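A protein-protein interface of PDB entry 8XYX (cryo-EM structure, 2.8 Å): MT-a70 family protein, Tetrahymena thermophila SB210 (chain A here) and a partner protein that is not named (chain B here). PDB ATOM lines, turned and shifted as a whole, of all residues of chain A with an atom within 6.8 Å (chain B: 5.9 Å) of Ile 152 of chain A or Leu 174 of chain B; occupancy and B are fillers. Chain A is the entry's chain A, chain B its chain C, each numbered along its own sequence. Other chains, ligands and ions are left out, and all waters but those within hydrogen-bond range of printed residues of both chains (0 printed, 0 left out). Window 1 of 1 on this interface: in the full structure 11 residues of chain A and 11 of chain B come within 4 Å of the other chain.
Leu 148 of chain A touches Leu 157 of chain B (CD1 to CD1, 3.7 Å).
CD2 of Leu 157 of chain B touches OD2 of Asp 151 of chain A (3.3 Å).
CD1 of Ile 152 of chain A touches CD2 of Leu 157 of chain B, at 3.7 Å.
Leu 174 of chain B touches Ile 152 of chain A (CD2 to CD1, 3.7 Å).
Lys 178 of chain B touches Ile 152 of chain A.
Leu 157 of chain B touches Arg 155 of chain A.
Arg 155 of chain A touches Leu 174 of chain B (CB to CD1, 3.7 Å).
CB of Leu 174 of chain B touches CG2 of Ile 156 of chain A, 3.6 Å away.
Tyr 159 of chain A touches Ile 170 of chain B.
Tyr 159 of chain A touches Leu 171 of chain B.
A ring nitrogen (ND1) of His 158 of chain A sits at hydrogen-bond distance from the guanidinium group of Arg 155 of chain A (3.5 Å).
Printed residues of chain B within 4 Å of Leu 148 of chain A: Leu 157.
Of chain B, only Leu 157, Leu 174, Leu 177 and Lys 178 come within 4 Å of Ile 152 of chain A.
Glu 153 of chain A touches none of the printed residues of chain B.
Printed residues of chain B within 4 Å of Ile 156 of chain A: Leu 174 (3.6 Å).
His 158 of chain A touches none of the printed residues of chain B.
Printed residues of chain A within 4 Å of Leu 157 of chain B: Leu 148 (3.7 Å), Asp 151 (3.3 Å), Ile 152 (3.7 Å) and Arg 155 (3.7 Å).
Of the printed residues of chain A, Ile 170 of chain B touches Tyr 159 (3.7 Å).
Of chain A, only Ile 152, Arg 155 and Ile 156 come within 4 Å of Leu 174 of chain B.
Of the printed residues of chain A, Lys 178 of chain B touches Ile 152 (3.7 Å).
The nearest residue of chain B that does not touch Ile 152 of chain A is Ile 160 of chain B (5.4 Å).
The nearest residue of chain A that does not touch Leu 174 of chain B is Tyr 159 of chain A (4.4 Å).
Printed residues of chain B that touch a printed residue of chain A: Leu 157, Ile 170, Leu 171, Leu 174, Leu 177 and Lys 178.
Hydrophobic or aromatic side chains of chain B that line the printed part of chain A: Leu 157, Ile 170, Leu 171, Leu 174 and Leu 177.
Of the 13 printed residues of chain A, 6 touch a printed residue of chain B.
Printed residues of chain A that touch a printed residue of chain B: Leu 148, Asp 151, Ile 152, Arg 155, Ile 156 and Tyr 159.
Hydrophobic or aromatic side chains of chain A that line the printed part of chain B: Leu 148, Ile 152, Ile 156 and Tyr 159.
Among the printed residues, no Asp or Glu carboxylate lies within 4 Å of a Lys or Arg side-chain nitrogen of the other chain.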
ATOM      1  N   GLY A 147      22.943   2.948 -30.777  1.00  0.00           N
ATOM      2  CA  GLY A 147      21.618   2.407 -30.514  1.00  0.00           C
ATOM      3  C   GLY A 147      21.652   1.226 -29.562  1.00  0.00           C
ATOM      4  O   GLY A 147      20.761   1.065 -28.723  1.00  0.00           O
ATOM      5  N   LEU A 148      22.688   0.392 -29.674  1.00  0.00           N
ATOM      6  CA  LEU A 148      22.867  -0.716 -28.741  1.00  0.00           C
ATOM      7  C   LEU A 148      23.099  -0.213 -27.323  1.00  0.00           C
ATOM      8  O   LEU A 148      22.580  -0.788 -26.361  1.00  0.00           O
ATOM      9  CB  LEU A 148      24.030  -1.597 -29.200  1.00  0.00           C
ATOM     10  CG  LEU A 148      24.367  -2.805 -28.327  1.00  0.00           C
ATOM     11  CD1 LEU A 148      23.184  -3.755 -28.259  1.00  0.00           C
ATOM     12  CD2 LEU A 148      25.602  -3.517 -28.856  1.00  0.00           C
ATOM     13  N   LEU A 149      23.882   0.859 -27.174  1.00  0.00           N
ATOM     14  CA  LEU A 149      24.118   1.442 -25.855  1.00  0.00           C
ATOM     15  C   LEU A 149      22.841   2.043 -25.277  1.00  0.00           C
ATOM     16  O   LEU A 149      22.576   1.915 -24.076  1.00  0.00           O
ATOM     17  CB  LEU A 149      25.223   2.494 -25.941  1.00  0.00           C
ATOM     18  CG  LEU A 149      25.450   3.383 -24.717  1.00  0.00           C
ATOM     19  CD1 LEU A 149      26.410   2.718 -23.747  1.00  0.00           C
ATOM     20  CD2 LEU A 149      25.968   4.750 -25.132  1.00  0.00           C
ATOM     21  N   GLN A 150      22.033   2.698 -26.117  1.00  0.00           N
ATOM     22  CA  GLN A 150      20.746   3.212 -25.650  1.00  0.00           C
ATOM     23  C   GLN A 150      19.825   2.079 -25.210  1.00  0.00           C
ATOM     24  O   GLN A 150      19.153   2.178 -24.173  1.00  0.00           O
ATOM     25  CB  GLN A 150      20.082   4.050 -26.744  1.00  0.00           C
ATOM     26  CG  GLN A 150      20.853   5.302 -27.130  1.00  0.00           C
ATOM     27  CD  GLN A 150      20.803   6.375 -26.062  1.00  0.00           C
ATOM     28  OE1 GLN A 150      21.776   6.595 -25.341  1.00  0.00           O
ATOM     29  NE2 GLN A 150      19.666   7.053 -25.958  1.00  0.00           N
ATOM     30  N   ASP A 151      19.794   0.987 -25.979  1.00  0.00           N
ATOM     31  CA  ASP A 151      18.965  -0.156 -25.608  1.00  0.00           C
ATOM     32  C   ASP A 151      19.468  -0.820 -24.331  1.00  0.00           C
ATOM     33  O   ASP A 151      18.668  -1.280 -23.511  1.00  0.00           O
ATOM     34  CB  ASP A 151      18.914  -1.165 -26.754  1.00  0.00           C
ATOM     35  CG  ASP A 151      17.980  -2.324 -26.466  1.00  0.00           C
ATOM     36  OD1 ASP A 151      16.790  -2.073 -26.179  1.00  0.00           O
ATOM     37  OD2 ASP A 151      18.432  -3.484 -26.531  1.00  0.00           O
ATOM     38  N   ILE A 152      20.789  -0.875 -24.141  1.00  0.00           N
ATOM     39  CA  ILE A 152      21.326  -1.469 -22.920  1.00  0.00           C
ATOM     40  C   ILE A 152      21.044  -0.571 -21.718  1.00  0.00           C
ATOM     41  O   ILE A 152      20.827  -1.068 -20.607  1.00  0.00           O
ATOM     42  CB  ILE A 152      22.828  -1.798 -23.094  1.00  0.00           C
ATOM     43  CG1 ILE A 152      23.167  -3.120 -22.408  1.00  0.00           C
ATOM     44  CG2 ILE A 152      23.743  -0.703 -22.564  1.00  0.00           C
ATOM     45  CD1 ILE A 152      22.437  -4.299 -22.979  1.00  0.00           C
ATOM     46  N   GLU A 153      21.000   0.752 -21.916  1.00  0.00           N
ATOM     47  CA  GLU A 153      20.602   1.644 -20.832  1.00  0.00           C
ATOM     48  C   GLU A 153      19.135   1.448 -20.474  1.00  0.00           C
ATOM     49  O   GLU A 153      18.773   1.415 -19.290  1.00  0.00           O
ATOM     50  CB  GLU A 153      20.875   3.096 -21.220  1.00  0.00           C
ATOM     51  CG  GLU A 153      20.841   4.066 -20.053  1.00  0.00           C
ATOM     52  CD  GLU A 153      22.099   4.905 -19.958  1.00  0.00           C
ATOM     53  OE1 GLU A 153      22.972   4.767 -20.840  1.00  0.00           O
ATOM     54  OE2 GLU A 153      22.216   5.700 -19.002  1.00  0.00           O
ATOM     55  N   LYS A 154      18.279   1.291 -21.487  1.00  0.00           N
ATOM     56  CA  LYS A 154      16.875   0.991 -21.225  1.00  0.00           C
ATOM     57  C   LYS A 154      16.721  -0.349 -20.514  1.00  0.00           C
ATOM     58  O   LYS A 154      15.865  -0.501 -19.635  1.00  0.00           O
ATOM     59  CB  LYS A 154      16.081   1.002 -22.532  1.00  0.00           C
ATOM     60  CG  LYS A 154      16.045   2.353 -23.227  1.00  0.00           C
ATOM     61  CD  LYS A 154      14.848   3.175 -22.786  1.00  0.00           C
ATOM     62  CE  LYS A 154      13.874   3.385 -23.935  1.00  0.00           C
ATOM     63  NZ  LYS A 154      14.435   4.282 -24.983  1.00  0.00           N
ATOM     64  N   ARG A 155      17.566  -1.323 -20.856  1.00  0.00           N
ATOM     65  CA  ARG A 155      17.457  -2.645 -20.246  1.00  0.00           C
ATOM     66  C   ARG A 155      17.935  -2.640 -18.798  1.00  0.00           C
ATOM     67  O   ARG A 155      17.332  -3.303 -17.945  1.00  0.00           O
ATOM     68  CB  ARG A 155      18.231  -3.671 -21.072  1.00  0.00           C
ATOM     69  CG  ARG A 155      17.498  -4.158 -22.317  1.00  0.00           C
ATOM     70  CD  ARG A 155      15.989  -4.223 -22.113  1.00  0.00           C
ATOM     71  NE  ARG A 155      15.561  -5.483 -21.519  1.00  0.00           N
ATOM     72  CZ  ARG A 155      14.335  -5.979 -21.622  1.00  0.00           C
ATOM     73  NH1 ARG A 155      13.387  -5.342 -22.291  1.00  0.00           N
ATOM     74  NH2 ARG A 155      14.053  -7.140 -21.038  1.00  0.00           N
ATOM     75  N   ILE A 156      19.014  -1.910 -18.492  1.00  0.00           N
ATOM     76  CA  ILE A 156      19.428  -1.821 -17.094  1.00  0.00           C
ATOM     77  C   ILE A 156      18.410  -1.024 -16.288  1.00  0.00           C
ATOM     78  O   ILE A 156      18.169  -1.334 -15.116  1.00  0.00           O
ATOM     79  CB  ILE A 156      20.857  -1.252 -16.933  1.00  0.00           C
ATOM     80  CG1 ILE A 156      20.949   0.224 -17.322  1.00  0.00           C
ATOM     81  CG2 ILE A 156      21.858  -2.073 -17.715  1.00  0.00           C
ATOM     82  CD1 ILE A 156      22.346   0.795 -17.234  1.00  0.00           C
ATOM     83  N   LEU A 157      17.771  -0.017 -16.897  1.00  0.00           N
ATOM     84  CA  LEU A 157      16.705   0.701 -16.203  1.00  0.00           C
ATOM     85  C   LEU A 157      15.510  -0.209 -15.935  1.00  0.00           C
ATOM     86  O   LEU A 157      14.869  -0.110 -14.881  1.00  0.00           O
ATOM     87  CB  LEU A 157      16.288   1.926 -17.018  1.00  0.00           C
ATOM     88  CG  LEU A 157      14.982   2.632 -16.650  1.00  0.00           C
ATOM     89  CD1 LEU A 157      15.088   3.281 -15.279  1.00  0.00           C
ATOM     90  CD2 LEU A 157      14.622   3.664 -17.706  1.00  0.00           C
ATOM     91  N   HIS A 158      15.198  -1.104 -16.875  1.00  0.00           N
ATOM     92  CA  HIS A 158      14.101  -2.044 -16.668  1.00  0.00           C
ATOM     93  C   HIS A 158      14.431  -3.066 -15.585  1.00  0.00           C
ATOM     94  O   HIS A 158      13.578  -3.386 -14.749  1.00  0.00           O
ATOM     95  CB  HIS A 158      13.760  -2.752 -17.980  1.00  0.00           C
ATOM     96  CG  HIS A 158      12.935  -3.988 -17.803  1.00  0.00           C
ATOM     97  ND1 HIS A 158      13.354  -5.230 -18.230  1.00  0.00           N
ATOM     98  CD2 HIS A 158      11.714  -4.175 -17.248  1.00  0.00           C
ATOM     99  CE1 HIS A 158      12.429  -6.127 -17.943  1.00  0.00           C
ATOM    100  NE2 HIS A 158      11.423  -5.513 -17.347  1.00  0.00           N
ATOM    101  N   TYR A 159      15.659  -3.592 -15.580  1.00  0.00           N
ATOM    102  CA  TYR A 159      16.002  -4.669 -14.658  1.00  0.00           C
ATOM    103  C   TYR A 159      16.359  -4.177 -13.259  1.00  0.00           C
ATOM    104  O   TYR A 159      16.245  -4.952 -12.300  1.00  0.00           O
ATOM    105  CB  TYR A 159      17.148  -5.506 -15.227  1.00  0.00           C
ATOM    106  CG  TYR A 159      16.665  -6.670 -16.059  1.00  0.00           C
ATOM    107  CD1 TYR A 159      16.386  -6.513 -17.411  1.00  0.00           C
ATOM    108  CD2 TYR A 159      16.464  -7.918 -15.489  1.00  0.00           C
ATOM    109  CE1 TYR A 159      15.936  -7.573 -18.173  1.00  0.00           C
ATOM    110  CE2 TYR A 159      16.013  -8.983 -16.243  1.00  0.00           C
ATOM    111  CZ  TYR A 159      15.750  -8.804 -17.584  1.00  0.00           C
ATOM    112  OH  TYR A 159      15.300  -9.862 -18.339  1.00  0.00           O
ATOM    113  N   LEU B 157      21.924  -9.547 -26.327  1.00  0.00           N
ATOM    114  CA  LEU B 157      20.914  -9.442 -25.280  1.00  0.00           C
ATOM    115  C   LEU B 157      20.117 -10.730 -25.128  1.00  0.00           C
ATOM    116  O   LEU B 157      19.618 -11.020 -24.035  1.00  0.00           O
ATOM    117  CB  LEU B 157      19.974  -8.276 -25.571  1.00  0.00           C
ATOM    118  CG  LEU B 157      20.570  -6.875 -25.460  1.00  0.00           C
ATOM    119  CD1 LEU B 157      20.873  -6.311 -26.836  1.00  0.00           C
ATOM    120  CD2 LEU B 157      19.616  -5.974 -24.709  1.00  0.00           C
ATOM    121  N   ILE B 160      21.955 -13.004 -22.732  1.00  0.00           N
ATOM    122  CA  ILE B 160      21.870 -12.551 -21.346  1.00  0.00           C
ATOM    123  C   ILE B 160      20.479 -12.812 -20.779  1.00  0.00           C
ATOM    124  O   ILE B 160      20.330 -13.321 -19.662  1.00  0.00           O
ATOM    125  CB  ILE B 160      22.247 -11.062 -21.252  1.00  0.00           C
ATOM    126  CG1 ILE B 160      23.681 -10.847 -21.735  1.00  0.00           C
ATOM    127  CG2 ILE B 160      22.080 -10.556 -19.834  1.00  0.00           C
ATOM    128  CD1 ILE B 160      24.029  -9.401 -21.966  1.00  0.00           C
ATOM    129  N   GLU B 169      22.755 -11.312 -11.703  1.00  0.00           N
ATOM    130  CA  GLU B 169      23.628 -11.798 -12.768  1.00  0.00           C
ATOM    131  C   GLU B 169      23.313 -11.119 -14.096  1.00  0.00           C
ATOM    132  O   GLU B 169      24.228 -10.749 -14.845  1.00  0.00           O
ATOM    133  CB  GLU B 169      23.496 -13.315 -12.900  1.00  0.00           C
ATOM    134  CG  GLU B 169      24.290 -14.103 -11.872  1.00  0.00           C
ATOM    135  CD  GLU B 169      23.772 -15.518 -11.703  1.00  0.00           C
ATOM    136  OE1 GLU B 169      22.732 -15.846 -12.312  1.00  0.00           O
ATOM    137  OE2 GLU B 169      24.401 -16.300 -10.961  1.00  0.00           O
ATOM    138  N   ILE B 170      22.023 -10.945 -14.399  1.00  0.00           N
ATOM    139  CA  ILE B 170      21.618 -10.250 -15.618  1.00  0.00           C
ATOM    140  C   ILE B 170      22.103  -8.808 -15.591  1.00  0.00           C
ATOM    141  O   ILE B 170      22.624  -8.298 -16.590  1.00  0.00           O
ATOM    142  CB  ILE B 170      20.090 -10.337 -15.799  1.00  0.00           C
ATOM    143  CG1 ILE B 170      19.670 -11.773 -16.112  1.00  0.00           C
ATOM    144  CG2 ILE B 170      19.614  -9.402 -16.899  1.00  0.00           C
ATOM    145  CD1 ILE B 170      18.193 -12.031 -15.925  1.00  0.00           C
ATOM    146  N   LEU B 171      21.963  -8.136 -14.445  1.00  0.00           N
ATOM    147  CA  LEU B 171      22.419  -6.754 -14.328  1.00  0.00           C
ATOM    148  C   LEU B 171      23.933  -6.651 -14.457  1.00  0.00           C
ATOM    149  O   LEU B 171      24.445  -5.698 -15.052  1.00  0.00           O
ATOM    150  CB  LEU B 171      21.953  -6.156 -13.002  1.00  0.00           C
ATOM    151  CG  LEU B 171      20.813  -5.142 -13.095  1.00  0.00           C
ATOM    152  CD1 LEU B 171      19.596  -5.617 -12.315  1.00  0.00           C
ATOM    153  CD2 LEU B 171      21.273  -3.783 -12.603  1.00  0.00           C
ATOM    154  N   THR B 172      24.668  -7.619 -13.902  1.00  0.00           N
ATOM    155  CA  THR B 172      26.122  -7.617 -14.033  1.00  0.00           C
ATOM    156  C   THR B 172      26.547  -7.806 -15.484  1.00  0.00           C
ATOM    157  O   THR B 172      27.450  -7.112 -15.970  1.00  0.00           O
ATOM    158  CB  THR B 172      26.729  -8.708 -13.148  1.00  0.00           C
ATOM    159  OG1 THR B 172      26.353  -8.483 -11.784  1.00  0.00           O
ATOM    160  CG2 THR B 172      28.246  -8.699 -13.247  1.00  0.00           C
ATOM    161  N   HIS B 173      25.895  -8.732 -16.195  1.00  0.00           N
ATOM    162  CA  HIS B 173      26.198  -8.930 -17.611  1.00  0.00           C
ATOM    163  C   HIS B 173      25.863  -7.689 -18.428  1.00  0.00           C
ATOM    164  O   HIS B 173      26.621  -7.302 -19.326  1.00  0.00           O
ATOM    165  CB  HIS B 173      25.438 -10.143 -18.147  1.00  0.00           C
ATOM    166  CG  HIS B 173      25.953 -11.452 -17.638  1.00  0.00           C
ATOM    167  ND1 HIS B 173      27.287 -11.675 -17.376  1.00  0.00           N
ATOM    168  CD2 HIS B 173      25.314 -12.608 -17.347  1.00  0.00           C
ATOM    169  CE1 HIS B 173      27.447 -12.912 -16.942  1.00  0.00           C
ATOM    170  NE2 HIS B 173      26.266 -13.500 -16.916  1.00  0.00           N
ATOM    171  N   LEU B 174      24.731  -7.048 -18.126  1.00  0.00           N
ATOM    172  CA  LEU B 174      24.340  -5.835 -18.837  1.00  0.00           C
ATOM    173  C   LEU B 174      25.319  -4.697 -18.577  1.00  0.00           C
ATOM    174  O   LEU B 174      25.662  -3.943 -19.494  1.00  0.00           O
ATOM    175  CB  LEU B 174      22.926  -5.431 -18.427  1.00  0.00           C
ATOM    176  CG  LEU B 174      21.749  -6.291 -18.895  1.00  0.00           C
ATOM    177  CD1 LEU B 174      20.443  -5.526 -18.787  1.00  0.00           C
ATOM    178  CD2 LEU B 174      21.961  -6.796 -20.311  1.00  0.00           C
ATOM    179  N   TYR B 175      25.781  -4.557 -17.332  1.00  0.00           N
ATOM    180  CA  TYR B 175      26.747  -3.512 -17.009  1.00  0.00           C
ATOM    181  C   TYR B 175      28.091  -3.774 -17.674  1.00  0.00           C
ATOM    182  O   TYR B 175      28.750  -2.836 -18.142  1.00  0.00           O
ATOM    183  CB  TYR B 175      26.907  -3.393 -15.495  1.00  0.00           C
ATOM    184  CG  TYR B 175      26.013  -2.346 -14.868  1.00  0.00           C
ATOM    185  CD1 TYR B 175      26.254  -0.993 -15.064  1.00  0.00           C
ATOM    186  CD2 TYR B 175      24.929  -2.712 -14.083  1.00  0.00           C
ATOM    187  CE1 TYR B 175      25.440  -0.033 -14.495  1.00  0.00           C
ATOM    188  CE2 TYR B 175      24.109  -1.760 -13.511  1.00  0.00           C
ATOM    189  CZ  TYR B 175      24.369  -0.423 -13.720  1.00  0.00           C
ATOM    190  OH  TYR B 175      23.555   0.528 -13.150  1.00  0.00           O
ATOM    191  N   ASN B 176      28.517  -5.041 -17.726  1.00  0.00           N
ATOM    192  CA  ASN B 176      29.751  -5.375 -18.434  1.00  0.00           C
ATOM    193  C   ASN B 176      29.631  -5.079 -19.924  1.00  0.00           C
ATOM    194  O   ASN B 176      30.572  -4.560 -20.538  1.00  0.00           O
ATOM    195  CB  ASN B 176      30.109  -6.842 -18.203  1.00  0.00           C
ATOM    196  CG  ASN B 176      31.101  -7.028 -17.072  1.00  0.00           C
ATOM    197  OD1 ASN B 176      31.740  -6.074 -16.627  1.00  0.00           O
ATOM    198  ND2 ASN B 176      31.235  -8.260 -16.599  1.00  0.00           N
ATOM    199  N   LEU B 177      28.478  -5.397 -20.521  1.00  0.00           N
ATOM    200  CA  LEU B 177      28.257  -5.086 -21.930  1.00  0.00           C
ATOM    201  C   LEU B 177      28.267  -3.581 -22.175  1.00  0.00           C
ATOM    202  O   LEU B 177      28.836  -3.113 -23.168  1.00  0.00           O
ATOM    203  CB  LEU B 177      26.938  -5.701 -22.399  1.00  0.00           C
ATOM    204  CG  LEU B 177      26.708  -5.840 -23.907  1.00  0.00           C
ATOM    205  CD1 LEU B 177      26.000  -7.147 -24.205  1.00  0.00           C
ATOM    206  CD2 LEU B 177      25.908  -4.670 -24.462  1.00  0.00           C
ATOM    207  N   LYS B 178      27.635  -2.811 -21.284  1.00  0.00           N
ATOM    208  CA  LYS B 178      27.629  -1.357 -21.422  1.00  0.00           C
ATOM    209  C   LYS B 178      29.036  -0.785 -21.304  1.00  0.00           C
ATOM    210  O   LYS B 178      29.416   0.112 -22.068  1.00  0.00           O
ATOM    211  CB  LYS B 178      26.708  -0.736 -20.371  1.00  0.00           C
ATOM    212  CG  LYS B 178      26.927   0.754 -20.149  1.00  0.00           C
ATOM    213  CD  LYS B 178      25.806   1.369 -19.332  1.00  0.00           C
ATOM    214  CE  LYS B 178      26.104   2.823 -19.003  1.00  0.00           C
ATOM    215  NZ  LYS B 178      27.279   2.955 -18.099  1.00  0.00           N
ATOM    216  N   ALA B 179      29.826  -1.299 -20.357  1.00  0.00           N
ATOM    217  CA  ALA B 179      31.206  -0.850 -20.211  1.00  0.00           C
ATOM    218  C   ALA B 179      32.030  -1.187 -21.446  1.00  0.00           C
ATOM    219  O   ALA B 179      32.849  -0.376 -21.894  1.00  0.00           O
ATOM    220  CB  ALA B 179      31.831  -1.471 -18.964  1.00  0.00           C
